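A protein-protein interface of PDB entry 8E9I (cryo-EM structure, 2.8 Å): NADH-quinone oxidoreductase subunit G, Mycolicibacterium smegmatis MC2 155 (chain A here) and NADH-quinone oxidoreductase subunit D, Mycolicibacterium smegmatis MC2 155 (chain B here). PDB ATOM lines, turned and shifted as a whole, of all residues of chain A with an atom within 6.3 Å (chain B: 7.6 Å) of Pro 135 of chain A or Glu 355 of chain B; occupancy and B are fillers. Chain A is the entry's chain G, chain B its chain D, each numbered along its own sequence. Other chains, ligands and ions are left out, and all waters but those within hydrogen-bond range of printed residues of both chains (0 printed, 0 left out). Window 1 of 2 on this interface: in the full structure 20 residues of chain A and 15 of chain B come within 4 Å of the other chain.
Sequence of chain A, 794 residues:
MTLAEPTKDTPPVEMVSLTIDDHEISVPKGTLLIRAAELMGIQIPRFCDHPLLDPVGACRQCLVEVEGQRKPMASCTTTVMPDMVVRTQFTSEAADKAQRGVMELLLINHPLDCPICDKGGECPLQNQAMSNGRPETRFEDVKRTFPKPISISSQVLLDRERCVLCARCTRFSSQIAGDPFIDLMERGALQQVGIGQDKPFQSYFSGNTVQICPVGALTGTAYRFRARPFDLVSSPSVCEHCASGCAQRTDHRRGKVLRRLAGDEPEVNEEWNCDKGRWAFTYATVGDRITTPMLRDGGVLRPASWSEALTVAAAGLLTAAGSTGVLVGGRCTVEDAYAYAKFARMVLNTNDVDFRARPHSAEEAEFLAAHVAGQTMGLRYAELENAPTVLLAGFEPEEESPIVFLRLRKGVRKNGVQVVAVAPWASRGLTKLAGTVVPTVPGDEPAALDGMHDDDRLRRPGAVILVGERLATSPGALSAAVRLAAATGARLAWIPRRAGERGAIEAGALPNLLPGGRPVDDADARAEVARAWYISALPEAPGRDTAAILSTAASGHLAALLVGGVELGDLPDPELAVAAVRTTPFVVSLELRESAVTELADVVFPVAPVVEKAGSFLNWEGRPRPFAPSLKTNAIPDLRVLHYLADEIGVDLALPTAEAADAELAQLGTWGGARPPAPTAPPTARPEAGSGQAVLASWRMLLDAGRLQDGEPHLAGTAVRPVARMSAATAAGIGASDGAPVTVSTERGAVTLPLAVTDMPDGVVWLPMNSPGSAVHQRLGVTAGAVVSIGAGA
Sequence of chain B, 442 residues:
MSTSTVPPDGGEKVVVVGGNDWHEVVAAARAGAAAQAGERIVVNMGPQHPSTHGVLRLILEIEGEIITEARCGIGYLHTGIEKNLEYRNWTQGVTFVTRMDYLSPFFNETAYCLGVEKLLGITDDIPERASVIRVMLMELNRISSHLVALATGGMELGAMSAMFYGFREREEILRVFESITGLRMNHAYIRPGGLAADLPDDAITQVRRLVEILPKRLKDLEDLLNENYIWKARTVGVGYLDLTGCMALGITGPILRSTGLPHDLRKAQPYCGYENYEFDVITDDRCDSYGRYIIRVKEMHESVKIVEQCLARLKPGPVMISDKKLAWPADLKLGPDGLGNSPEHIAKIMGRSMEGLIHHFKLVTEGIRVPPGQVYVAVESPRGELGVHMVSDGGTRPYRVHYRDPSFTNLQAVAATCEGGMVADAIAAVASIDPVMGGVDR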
ATOM      1  N   ARG A 100      -6.985  -5.836  27.626  1.00  0.00           N
ATOM      2  CA  ARG A 100      -7.515  -7.015  26.952  1.00  0.00           C
ATOM      3  C   ARG A 100      -8.859  -6.718  26.302  1.00  0.00           C
ATOM      4  O   ARG A 100      -9.151  -7.216  25.210  1.00  0.00           O
ATOM      5  CB  ARG A 100      -7.626  -8.170  27.940  1.00  0.00           C
ATOM      6  CG  ARG A 100      -6.290  -8.800  28.252  1.00  0.00           C
ATOM      7  CD  ARG A 100      -6.401  -9.868  29.310  1.00  0.00           C
ATOM      8  NE  ARG A 100      -5.090 -10.363  29.710  1.00  0.00           N
ATOM      9  CZ  ARG A 100      -4.399 -11.281  29.051  1.00  0.00           C
ATOM     10  NH1 ARG A 100      -4.864 -11.836  27.944  1.00  0.00           N
ATOM     11  NH2 ARG A 100      -3.208 -11.648  29.512  1.00  0.00           N
ATOM     12  N   MET A 103      -8.185  -4.902  23.219  1.00  0.00           N
ATOM     13  CA  MET A 103      -7.698  -5.842  22.217  1.00  0.00           C
ATOM     14  C   MET A 103      -8.856  -6.578  21.561  1.00  0.00           C
ATOM     15  O   MET A 103      -8.929  -6.673  20.328  1.00  0.00           O
ATOM     16  CB  MET A 103      -6.737  -6.833  22.870  1.00  0.00           C
ATOM     17  CG  MET A 103      -6.112  -7.825  21.920  1.00  0.00           C
ATOM     18  SD  MET A 103      -4.712  -7.092  21.064  1.00  0.00           S
ATOM     19  CE  MET A 103      -5.451  -6.743  19.483  1.00  0.00           C
ATOM     20  N   GLU A 104      -9.774  -7.105  22.371  1.00  0.00           N
ATOM     21  CA  GLU A 104     -10.933  -7.800  21.823  1.00  0.00           C
ATOM     22  C   GLU A 104     -11.710  -6.896  20.882  1.00  0.00           C
ATOM     23  O   GLU A 104     -11.984  -7.262  19.735  1.00  0.00           O
ATOM     24  CB  GLU A 104     -11.838  -8.291  22.948  1.00  0.00           C
ATOM     25  CG  GLU A 104     -13.240  -8.651  22.497  1.00  0.00           C
ATOM     26  CD  GLU A 104     -14.081  -9.188  23.622  1.00  0.00           C
ATOM     27  OE1 GLU A 104     -14.086  -8.573  24.705  1.00  0.00           O
ATOM     28  OE2 GLU A 104     -14.748 -10.220  23.424  1.00  0.00           O
ATOM     29  N   LEU A 105     -12.069  -5.703  21.348  1.00  0.00           N
ATOM     30  CA  LEU A 105     -12.788  -4.778  20.484  1.00  0.00           C
ATOM     31  C   LEU A 105     -11.992  -4.470  19.228  1.00  0.00           C
ATOM     32  O   LEU A 105     -12.571  -4.178  18.178  1.00  0.00           O
ATOM     33  CB  LEU A 105     -13.099  -3.496  21.245  1.00  0.00           C
ATOM     34  CG  LEU A 105     -14.072  -3.671  22.403  1.00  0.00           C
ATOM     35  CD1 LEU A 105     -14.251  -2.363  23.128  1.00  0.00           C
ATOM     36  CD2 LEU A 105     -15.397  -4.193  21.901  1.00  0.00           C
ATOM     37  N   LEU A 107     -10.154  -6.643  17.635  1.00  0.00           N
ATOM     38  CA  LEU A 107     -10.136  -7.799  16.751  1.00  0.00           C
ATOM     39  C   LEU A 107     -11.503  -8.202  16.219  1.00  0.00           C
ATOM     40  O   LEU A 107     -11.564  -8.988  15.270  1.00  0.00           O
ATOM     41  CB  LEU A 107      -9.517  -9.001  17.462  1.00  0.00           C
ATOM     42  CG  LEU A 107      -7.998  -8.986  17.577  1.00  0.00           C
ATOM     43  CD1 LEU A 107      -7.524 -10.198  18.346  1.00  0.00           C
ATOM     44  CD2 LEU A 107      -7.357  -8.941  16.211  1.00  0.00           C
ATOM     45  N   ILE A 108     -12.601  -7.702  16.787  1.00  0.00           N
ATOM     46  CA  ILE A 108     -13.907  -8.224  16.390  1.00  0.00           C
ATOM     47  C   ILE A 108     -14.160  -7.977  14.910  1.00  0.00           C
ATOM     48  O   ILE A 108     -14.622  -8.870  14.193  1.00  0.00           O
ATOM     49  CB  ILE A 108     -15.032  -7.635  17.262  1.00  0.00           C
ATOM     50  CG1 ILE A 108     -15.104  -6.117  17.138  1.00  0.00           C
ATOM     51  CG2 ILE A 108     -14.850  -8.048  18.695  1.00  0.00           C
ATOM     52  CD1 ILE A 108     -16.100  -5.502  18.072  1.00  0.00           C
ATOM     53  N   ALA A 129      -1.954  -9.405  20.230  1.00  0.00           N
ATOM     54  CA  ALA A 129      -3.121 -10.218  20.539  1.00  0.00           C
ATOM     55  C   ALA A 129      -2.711 -11.534  21.176  1.00  0.00           C
ATOM     56  O   ALA A 129      -3.467 -12.101  21.971  1.00  0.00           O
ATOM     57  CB  ALA A 129      -3.938 -10.469  19.275  1.00  0.00           C
ATOM     58  N   MET A 130      -1.530 -12.042  20.829  1.00  0.00           N
ATOM     59  CA  MET A 130      -0.986 -13.189  21.544  1.00  0.00           C
ATOM     60  C   MET A 130      -0.641 -12.819  22.978  1.00  0.00           C
ATOM     61  O   MET A 130      -1.049 -13.497  23.926  1.00  0.00           O
ATOM     62  CB  MET A 130       0.253 -13.721  20.825  1.00  0.00           C
ATOM     63  CG  MET A 130      -0.025 -14.581  19.617  1.00  0.00           C
ATOM     64  SD  MET A 130      -1.319 -15.790  19.908  1.00  0.00           S
ATOM     65  CE  MET A 130      -0.339 -17.261  20.153  1.00  0.00           C
ATOM     66  N   GLY A 133      -4.147 -10.747  24.491  1.00  0.00           N
ATOM     67  CA  GLY A 133      -5.469 -11.028  23.984  1.00  0.00           C
ATOM     68  C   GLY A 133      -6.107 -12.249  24.624  1.00  0.00           C
ATOM     69  O   GLY A 133      -5.460 -13.069  25.265  1.00  0.00           O
ATOM     70  N   ARG A 134      -7.410 -12.350  24.429  1.00  0.00           N
ATOM     71  CA  ARG A 134      -8.156 -13.514  24.857  1.00  0.00           C
ATOM     72  C   ARG A 134      -7.797 -14.710  23.985  1.00  0.00           C
ATOM     73  O   ARG A 134      -7.385 -14.550  22.836  1.00  0.00           O
ATOM     74  CB  ARG A 134      -9.651 -13.227  24.776  1.00  0.00           C
ATOM     75  CG  ARG A 134     -10.066 -11.989  25.549  1.00  0.00           C
ATOM     76  CD  ARG A 134     -11.559 -11.701  25.460  1.00  0.00           C
ATOM     77  NE  ARG A 134     -12.381 -12.862  25.778  1.00  0.00           N
ATOM     78  CZ  ARG A 134     -12.795 -13.753  24.892  1.00  0.00           C
ATOM     79  NH1 ARG A 134     -12.445 -13.676  23.619  1.00  0.00           N
ATOM     80  NH2 ARG A 134     -13.574 -14.750  25.293  1.00  0.00           N
ATOM     81  N   PRO A 135      -7.925 -15.928  24.511  1.00  0.00           N
ATOM     82  CA  PRO A 135      -7.614 -17.101  23.683  1.00  0.00           C
ATOM     83  C   PRO A 135      -8.455 -17.216  22.423  1.00  0.00           C
ATOM     84  O   PRO A 135      -7.918 -17.601  21.378  1.00  0.00           O
ATOM     85  CB  PRO A 135      -7.869 -18.276  24.636  1.00  0.00           C
ATOM     86  CG  PRO A 135      -8.803 -17.734  25.664  1.00  0.00           C
ATOM     87  CD  PRO A 135      -8.393 -16.313  25.852  1.00  0.00           C
ATOM     88  N   GLU A 136      -9.746 -16.887  22.473  1.00  0.00           N
ATOM     89  CA  GLU A 136     -10.635 -17.147  21.348  1.00  0.00           C
ATOM     90  C   GLU A 136     -11.665 -16.034  21.232  1.00  0.00           C
ATOM     91  O   GLU A 136     -11.832 -15.222  22.143  1.00  0.00           O
ATOM     92  CB  GLU A 136     -11.339 -18.499  21.496  1.00  0.00           C
ATOM     93  N   THR A 137     -12.355 -16.005  20.094  1.00  0.00           N
ATOM     94  CA  THR A 137     -13.382 -14.995  19.884  1.00  0.00           C
ATOM     95  C   THR A 137     -14.529 -15.148  20.867  1.00  0.00           C
ATOM     96  O   THR A 137     -14.909 -16.252  21.263  1.00  0.00           O
ATOM     97  CB  THR A 137     -13.959 -15.046  18.465  1.00  0.00           C
ATOM     98  OG1 THR A 137     -14.452 -16.362  18.176  1.00  0.00           O
ATOM     99  CG2 THR A 137     -12.968 -14.587  17.434  1.00  0.00           C
ATOM    100  N   ARG A 138     -15.072 -14.003  21.256  1.00  0.00           N
ATOM    101  CA  ARG A 138     -16.369 -13.899  21.885  1.00  0.00           C
ATOM    102  C   ARG A 138     -17.401 -13.297  20.944  1.00  0.00           C
ATOM    103  O   ARG A 138     -18.580 -13.225  21.306  1.00  0.00           O
ATOM    104  CB  ARG A 138     -16.259 -13.036  23.147  1.00  0.00           C
ATOM    105  CG  ARG A 138     -17.464 -13.038  24.047  1.00  0.00           C
ATOM    106  CD  ARG A 138     -17.032 -12.737  25.463  1.00  0.00           C
ATOM    107  NE  ARG A 138     -16.286 -11.487  25.533  1.00  0.00           N
ATOM    108  CZ  ARG A 138     -16.041 -10.822  26.651  1.00  0.00           C
ATOM    109  NH1 ARG A 138     -16.443 -11.272  27.827  1.00  0.00           N
ATOM    110  NH2 ARG A 138     -15.369  -9.676  26.591  1.00  0.00           N
ATOM    111  N   PHE A 139     -16.992 -12.887  19.747  1.00  0.00           N
ATOM    112  CA  PHE A 139     -17.823 -12.118  18.830  1.00  0.00           C
ATOM    113  C   PHE A 139     -18.475 -13.059  17.828  1.00  0.00           C
ATOM    114  O   PHE A 139     -17.830 -13.504  16.876  1.00  0.00           O
ATOM    115  CB  PHE A 139     -16.960 -11.074  18.127  1.00  0.00           C
ATOM    116  CG  PHE A 139     -17.674 -10.288  17.073  1.00  0.00           C
ATOM    117  CD1 PHE A 139     -18.411  -9.172  17.400  1.00  0.00           C
ATOM    118  CD2 PHE A 139     -17.578 -10.649  15.746  1.00  0.00           C
ATOM    119  CE1 PHE A 139     -19.053  -8.443  16.428  1.00  0.00           C
ATOM    120  CE2 PHE A 139     -18.218  -9.923  14.772  1.00  0.00           C
ATOM    121  CZ  PHE A 139     -18.959  -8.820  15.115  1.00  0.00           C
ATOM    122  N   SER B 322      -4.640 -26.894  28.226  1.00  0.00           N
ATOM    123  CA  SER B 322      -5.800 -26.102  27.844  1.00  0.00           C
ATOM    124  C   SER B 322      -5.474 -24.629  27.658  1.00  0.00           C
ATOM    125  O   SER B 322      -6.324 -23.881  27.164  1.00  0.00           O
ATOM    126  CB  SER B 322      -6.906 -26.254  28.886  1.00  0.00           C
ATOM    127  OG  SER B 322      -6.457 -25.875  30.172  1.00  0.00           O
ATOM    128  N   ASP B 323      -4.276 -24.191  28.035  1.00  0.00           N
ATOM    129  CA  ASP B 323      -3.873 -22.802  27.837  1.00  0.00           C
ATOM    130  C   ASP B 323      -3.610 -22.573  26.358  1.00  0.00           C
ATOM    131  O   ASP B 323      -2.559 -22.941  25.835  1.00  0.00           O
ATOM    132  CB  ASP B 323      -2.640 -22.479  28.670  1.00  0.00           C
ATOM    133  CG  ASP B 323      -2.353 -20.996  28.727  1.00  0.00           C
ATOM    134  OD1 ASP B 323      -2.969 -20.240  27.945  1.00  0.00           O
ATOM    135  OD2 ASP B 323      -1.523 -20.578  29.560  1.00  0.00           O
ATOM    136  N   LYS B 324      -4.566 -21.944  25.675  1.00  0.00           N
ATOM    137  CA  LYS B 324      -4.455 -21.764  24.235  1.00  0.00           C
ATOM    138  C   LYS B 324      -3.249 -20.926  23.837  1.00  0.00           C
ATOM    139  O   LYS B 324      -2.822 -21.005  22.682  1.00  0.00           O
ATOM    140  CB  LYS B 324      -5.734 -21.126  23.693  1.00  0.00           C
ATOM    141  N   LYS B 325      -2.687 -20.144  24.752  1.00  0.00           N
ATOM    142  CA  LYS B 325      -1.520 -19.325  24.452  1.00  0.00           C
ATOM    143  C   LYS B 325      -0.281 -20.150  24.151  1.00  0.00           C
ATOM    144  O   LYS B 325       0.675 -19.613  23.585  1.00  0.00           O
ATOM    145  CB  LYS B 325      -1.216 -18.384  25.620  1.00  0.00           C
ATOM    146  CG  LYS B 325      -2.281 -17.332  25.882  1.00  0.00           C
ATOM    147  CD  LYS B 325      -2.342 -16.313  24.768  1.00  0.00           C
ATOM    148  CE  LYS B 325      -3.273 -15.165  25.119  1.00  0.00           C
ATOM    149  NZ  LYS B 325      -4.686 -15.599  25.229  1.00  0.00           N
ATOM    150  N   LYS B 348     -13.050 -23.000  12.023  1.00  0.00           N
ATOM    151  CA  LYS B 348     -12.894 -22.140  13.188  1.00  0.00           C
ATOM    152  C   LYS B 348     -11.956 -20.981  12.891  1.00  0.00           C
ATOM    153  O   LYS B 348     -12.279 -19.820  13.160  1.00  0.00           O
ATOM    154  CB  LYS B 348     -12.368 -22.954  14.366  1.00  0.00           C
ATOM    155  CG  LYS B 348     -12.365 -22.196  15.673  1.00  0.00           C
ATOM    156  CD  LYS B 348     -11.723 -22.998  16.788  1.00  0.00           C
ATOM    157  CE  LYS B 348     -10.213 -23.028  16.644  1.00  0.00           C
ATOM    158  NZ  LYS B 348      -9.528 -23.181  17.956  1.00  0.00           N
ATOM    159  N   ILE B 349     -10.784 -21.276  12.326  1.00  0.00           N
ATOM    160  CA  ILE B 349      -9.758 -20.241  12.244  1.00  0.00           C
ATOM    161  C   ILE B 349      -9.872 -19.421  10.963  1.00  0.00           C
ATOM    162  O   ILE B 349      -9.274 -18.345  10.871  1.00  0.00           O
ATOM    163  CB  ILE B 349      -8.345 -20.838  12.379  1.00  0.00           C
ATOM    164  CG1 ILE B 349      -7.933 -21.576  11.107  1.00  0.00           C
ATOM    165  CG2 ILE B 349      -8.269 -21.755  13.579  1.00  0.00           C
ATOM    166  CD1 ILE B 349      -6.572 -22.200  11.199  1.00  0.00           C
ATOM    167  N   ARG B 352     -14.520 -18.045  11.481  1.00  0.00           N
ATOM    168  CA  ARG B 352     -15.131 -17.546  12.703  1.00  0.00           C
ATOM    169  C   ARG B 352     -14.160 -16.830  13.636  1.00  0.00           C
ATOM    170  O   ARG B 352     -14.364 -15.657  13.958  1.00  0.00           O
ATOM    171  CB  ARG B 352     -15.797 -18.702  13.450  1.00  0.00           C
ATOM    172  N   SER B 353     -13.100 -17.509  14.070  1.00  0.00           N
ATOM    173  CA  SER B 353     -12.351 -17.101  15.256  1.00  0.00           C
ATOM    174  C   SER B 353     -11.094 -16.331  14.858  1.00  0.00           C
ATOM    175  O   SER B 353     -10.100 -16.932  14.444  1.00  0.00           O
ATOM    176  CB  SER B 353     -11.992 -18.323  16.094  1.00  0.00           C
ATOM    177  OG  SER B 353     -11.522 -17.944  17.373  1.00  0.00           O
ATOM    178  N   MET B 354     -11.127 -15.006  15.009  1.00  0.00           N
ATOM    179  CA  MET B 354      -9.948 -14.202  14.702  1.00  0.00           C
ATOM    180  C   MET B 354      -8.819 -14.465  15.688  1.00  0.00           C
ATOM    181  O   MET B 354      -7.666 -14.655  15.288  1.00  0.00           O
ATOM    182  CB  MET B 354     -10.298 -12.718  14.689  1.00  0.00           C
ATOM    183  CG  MET B 354      -9.150 -11.844  14.229  1.00  0.00           C
ATOM    184  SD  MET B 354      -8.731 -12.144  12.515  1.00  0.00           S
ATOM    185  CE  MET B 354      -7.033 -11.596  12.470  1.00  0.00           C
ATOM    186  N   GLU B 355      -9.116 -14.449  16.987  1.00  0.00           N
ATOM    187  CA  GLU B 355      -8.090 -14.820  17.955  1.00  0.00           C
ATOM    188  C   GLU B 355      -7.602 -16.237  17.709  1.00  0.00           C
ATOM    189  O   GLU B 355      -6.411 -16.527  17.864  1.00  0.00           O
ATOM    190  CB  GLU B 355      -8.614 -14.663  19.382  1.00  0.00           C
ATOM    191  CG  GLU B 355      -8.807 -13.215  19.825  1.00  0.00           C
ATOM    192  CD  GLU B 355     -10.089 -12.594  19.324  1.00  0.00           C
ATOM    193  OE1 GLU B 355     -10.872 -13.296  18.669  1.00  0.00           O
ATOM    194  OE2 GLU B 355     -10.321 -11.403  19.598  1.00  0.00           O
ATOM    195  N   GLY B 356      -8.503 -17.134  17.311  1.00  0.00           N
ATOM    196  CA  GLY B 356      -8.075 -18.471  16.955  1.00  0.00           C
ATOM    197  C   GLY B 356      -7.099 -18.467  15.798  1.00  0.00           C
ATOM    198  O   GLY B 356      -6.088 -19.172  15.822  1.00  0.00           O
ATOM    199  N   LEU B 357      -7.385 -17.667  14.773  1.00  0.00           N
ATOM    200  CA  LEU B 357      -6.486 -17.582  13.631  1.00  0.00           C
ATOM    201  C   LEU B 357      -5.131 -17.036  14.046  1.00  0.00           C
ATOM    202  O   LEU B 357      -4.092 -17.558  13.632  1.00  0.00           O
ATOM    203  CB  LEU B 357      -7.104 -16.704  12.550  1.00  0.00           C
ATOM    204  CG  LEU B 357      -6.307 -16.551  11.256  1.00  0.00           C
ATOM    205  CD1 LEU B 357      -5.986 -17.902  10.654  1.00  0.00           C
ATOM    206  CD2 LEU B 357      -7.087 -15.714  10.272  1.00  0.00           C
ATOM    207  N   ILE B 358      -5.120 -15.983  14.859  1.00  0.00           N
ATOM    208  CA  ILE B 358      -3.854 -15.396  15.280  1.00  0.00           C
ATOM    209  C   ILE B 358      -3.046 -16.411  16.068  1.00  0.00           C
ATOM    210  O   ILE B 358      -1.830 -16.532  15.893  1.00  0.00           O
ATOM    211  CB  ILE B 358      -4.096 -14.117  16.098  1.00  0.00           C
ATOM    212  CG1 ILE B 358      -4.613 -13.009  15.189  1.00  0.00           C
ATOM    213  CG2 ILE B 358      -2.817 -13.689  16.789  1.00  0.00           C
ATOM    214  CD1 ILE B 358      -5.080 -11.782  15.928  1.00  0.00           C
ATOM    215  N   HIS B 359      -3.705 -17.141  16.966  1.00  0.00           N
ATOM    216  CA  HIS B 359      -2.989 -18.113  17.778  1.00  0.00           C
ATOM    217  C   HIS B 359      -2.435 -19.240  16.926  1.00  0.00           C
ATOM    218  O   HIS B 359      -1.281 -19.641  17.096  1.00  0.00           O
ATOM    219  CB  HIS B 359      -3.903 -18.651  18.870  1.00  0.00           C
ATOM    220  CG  HIS B 359      -4.067 -17.708  20.015  1.00  0.00           C
ATOM    221  ND1 HIS B 359      -4.761 -16.525  19.908  1.00  0.00           N
ATOM    222  CD2 HIS B 359      -3.613 -17.763  21.287  1.00  0.00           C
ATOM    223  CE1 HIS B 359      -4.734 -15.894  21.066  1.00  0.00           C
ATOM    224  NE2 HIS B 359      -4.043 -16.624  21.920  1.00  0.00           N
ATOM    225  N   HIS B 360      -3.234 -19.764  16.001  1.00  0.00           N
ATOM    226  CA  HIS B 360      -2.718 -20.786  15.101  1.00  0.00           C
ATOM    227  C   HIS B 360      -1.499 -20.267  14.353  1.00  0.00           C
ATOM    228  O   HIS B 360      -0.432 -20.896  14.349  1.00  0.00           O
ATOM    229  CB  HIS B 360      -3.805 -21.213  14.121  1.00  0.00           C
ATOM    230  CG  HIS B 360      -3.331 -22.178  13.086  1.00  0.00           C
ATOM    231  ND1 HIS B 360      -3.358 -23.541  13.275  1.00  0.00           N
ATOM    232  CD2 HIS B 360      -2.798 -21.979  11.859  1.00  0.00           C
ATOM    233  CE1 HIS B 360      -2.877 -24.142  12.204  1.00  0.00           C
ATOM    234  NE2 HIS B 360      -2.527 -23.216  11.330  1.00  0.00           N
ATOM    235  N   PHE B 361      -1.634 -19.089  13.749  1.00  0.00           N
ATOM    236  CA  PHE B 361      -0.567 -18.517  12.941  1.00  0.00           C
ATOM    237  C   PHE B 361       0.709 -18.348  13.758  1.00  0.00           C
ATOM    238  O   PHE B 361       1.796 -18.737  13.324  1.00  0.00           O
ATOM    239  CB  PHE B 361      -1.053 -17.180  12.379  1.00  0.00           C
ATOM    240  CG  PHE B 361      -0.177 -16.599  11.317  1.00  0.00           C
ATOM    241  CD1 PHE B 361       1.071 -16.099  11.619  1.00  0.00           C
ATOM    242  CD2 PHE B 361      -0.617 -16.529  10.016  1.00  0.00           C
ATOM    243  CE1 PHE B 361       1.862 -15.554  10.643  1.00  0.00           C
ATOM    244  CE2 PHE B 361       0.167 -15.983   9.037  1.00  0.00           C
ATOM    245  CZ  PHE B 361       1.410 -15.498   9.350  1.00  0.00           C
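SD of Met 130 of chain A lies close to NE2 of His 359 of chain B, at 3.5 Å. The side-chain hydroxyl of Ser 353 of chain B sits at hydrogen-bond distance from the side-chain hydroxyl of Thr 137 of chain A (3.4 Å). The backbone carbonyl oxygen of Gly 133 of chain A sits at hydrogen-bond distance from the side-chain amino group of Lys 325 of chain B, at 2.6 Å. The backbone NH of Thr 137 of chain A sits close to the side-chain carboxylate of Glu 355 of chain B, 3.4 Å away. The side-chain amino group of Lys 325 of chain B lies close to the backbone nitrogen of Pro 135 of chain A (3.3 Å).
SD of Met 103 of chain A lies close to N of Ala 129 of chain A, at 3.7 Å. The backbone carbonyl oxygen (O) of Glu 355 of chain B sits at hydrogen-bond distance from a ring nitrogen (ND1) of His 359 of chain B (2.6 Å). The backbone carbonyl oxygen (O) of Lys 348 of chain B is in hydrogen-bond range of the backbone NH (N) of Ser 353 of chain B, 2.6 Å away. N of Gly 356 of chain B sits at hydrogen-bond distance from OG of Ser 353 of chain B, 3.1 Å away. OD1 of Asp 323 of chain B lies close to N of Lys 325 of chain B (3.2 Å). NH1 of Arg 100 of chain A lies within hydrogen-bond range of O of Gly 133 of chain A (3.0 Å).
CG of Met 354 of chain B touches O of Leu 107 of chain A, at 3.9 Å. Glu 355 of chain B touches Leu 107 of chain A (OE2 to CD1, 3.3 Å). CD2 of Leu 107 of chain A touches CD1 of Ile 358 of chain B, 3.7 Å away. Met 130 of chain A touches Lys 325 of chain B (O to CE, 3.0 Å). Arg 134 of chain A touches His 359 of chain B (O to CE1, 3.5 Å). Pro 135 of chain A touches Glu 355 of chain B (O to CB, 3.6 Å). Pro 135 of chain A touches His 359 of chain B. Glu 136 of chain A touches Glu 355 of chain B (CA to CB, 3.8 Å). Arg 352 of chain B touches Thr 137 of chain A (O to CG2, 3.9 Å). Thr 137 of chain A touches Met 354 of chain B (CG2 to N, 3.1 Å).
Of chain B, only Lys 324, Lys 325, Glu 355 and His 359 come within 4 Å of Pro 135 of chain A. Glu 355 of chain B touches five residues of chain A. Printed residues of chain A within 4 Å of Arg 352 of chain B: Thr 137 (3.9 Å). Of the printed residues of chain A, Lys 324 of chain B touches Pro 135 (3.7 Å). The nearest residue of chain B that does not touch Pro 135 of chain A is Gly 356 of chain B (4.1 Å). The nearest residue of chain A that does not touch Glu 355 of chain B is Glu 104 of chain A (4.3 Å).
Printed residues of chain A that touch a printed residue of chain B: Leu 107, Ala 129, Met 130, Gly 133, Arg 134, Pro 135, Glu 136 and Thr 137. Hydrophobic or aromatic side chains of chain A within 4 Å of the printed part of chain B: Leu 107, Ala 129, Met 130 and Pro 135. Printed residues of chain B that touch a printed residue of chain A: Lys 324, Lys 325, Arg 352, Ser 353, Met 354, Glu 355, Ile 358 and His 359. Hydrophobic or aromatic side chains of chain B that line the printed part of chain A: Met 354, Ile 358 and His 359. Among the printed residues, 19 pairs touch across the chains. Among the printed residues, no Asp or Glu carboxylate lies within 4 Å of a Lys or Arg side-chain nitrogen of the other chain.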
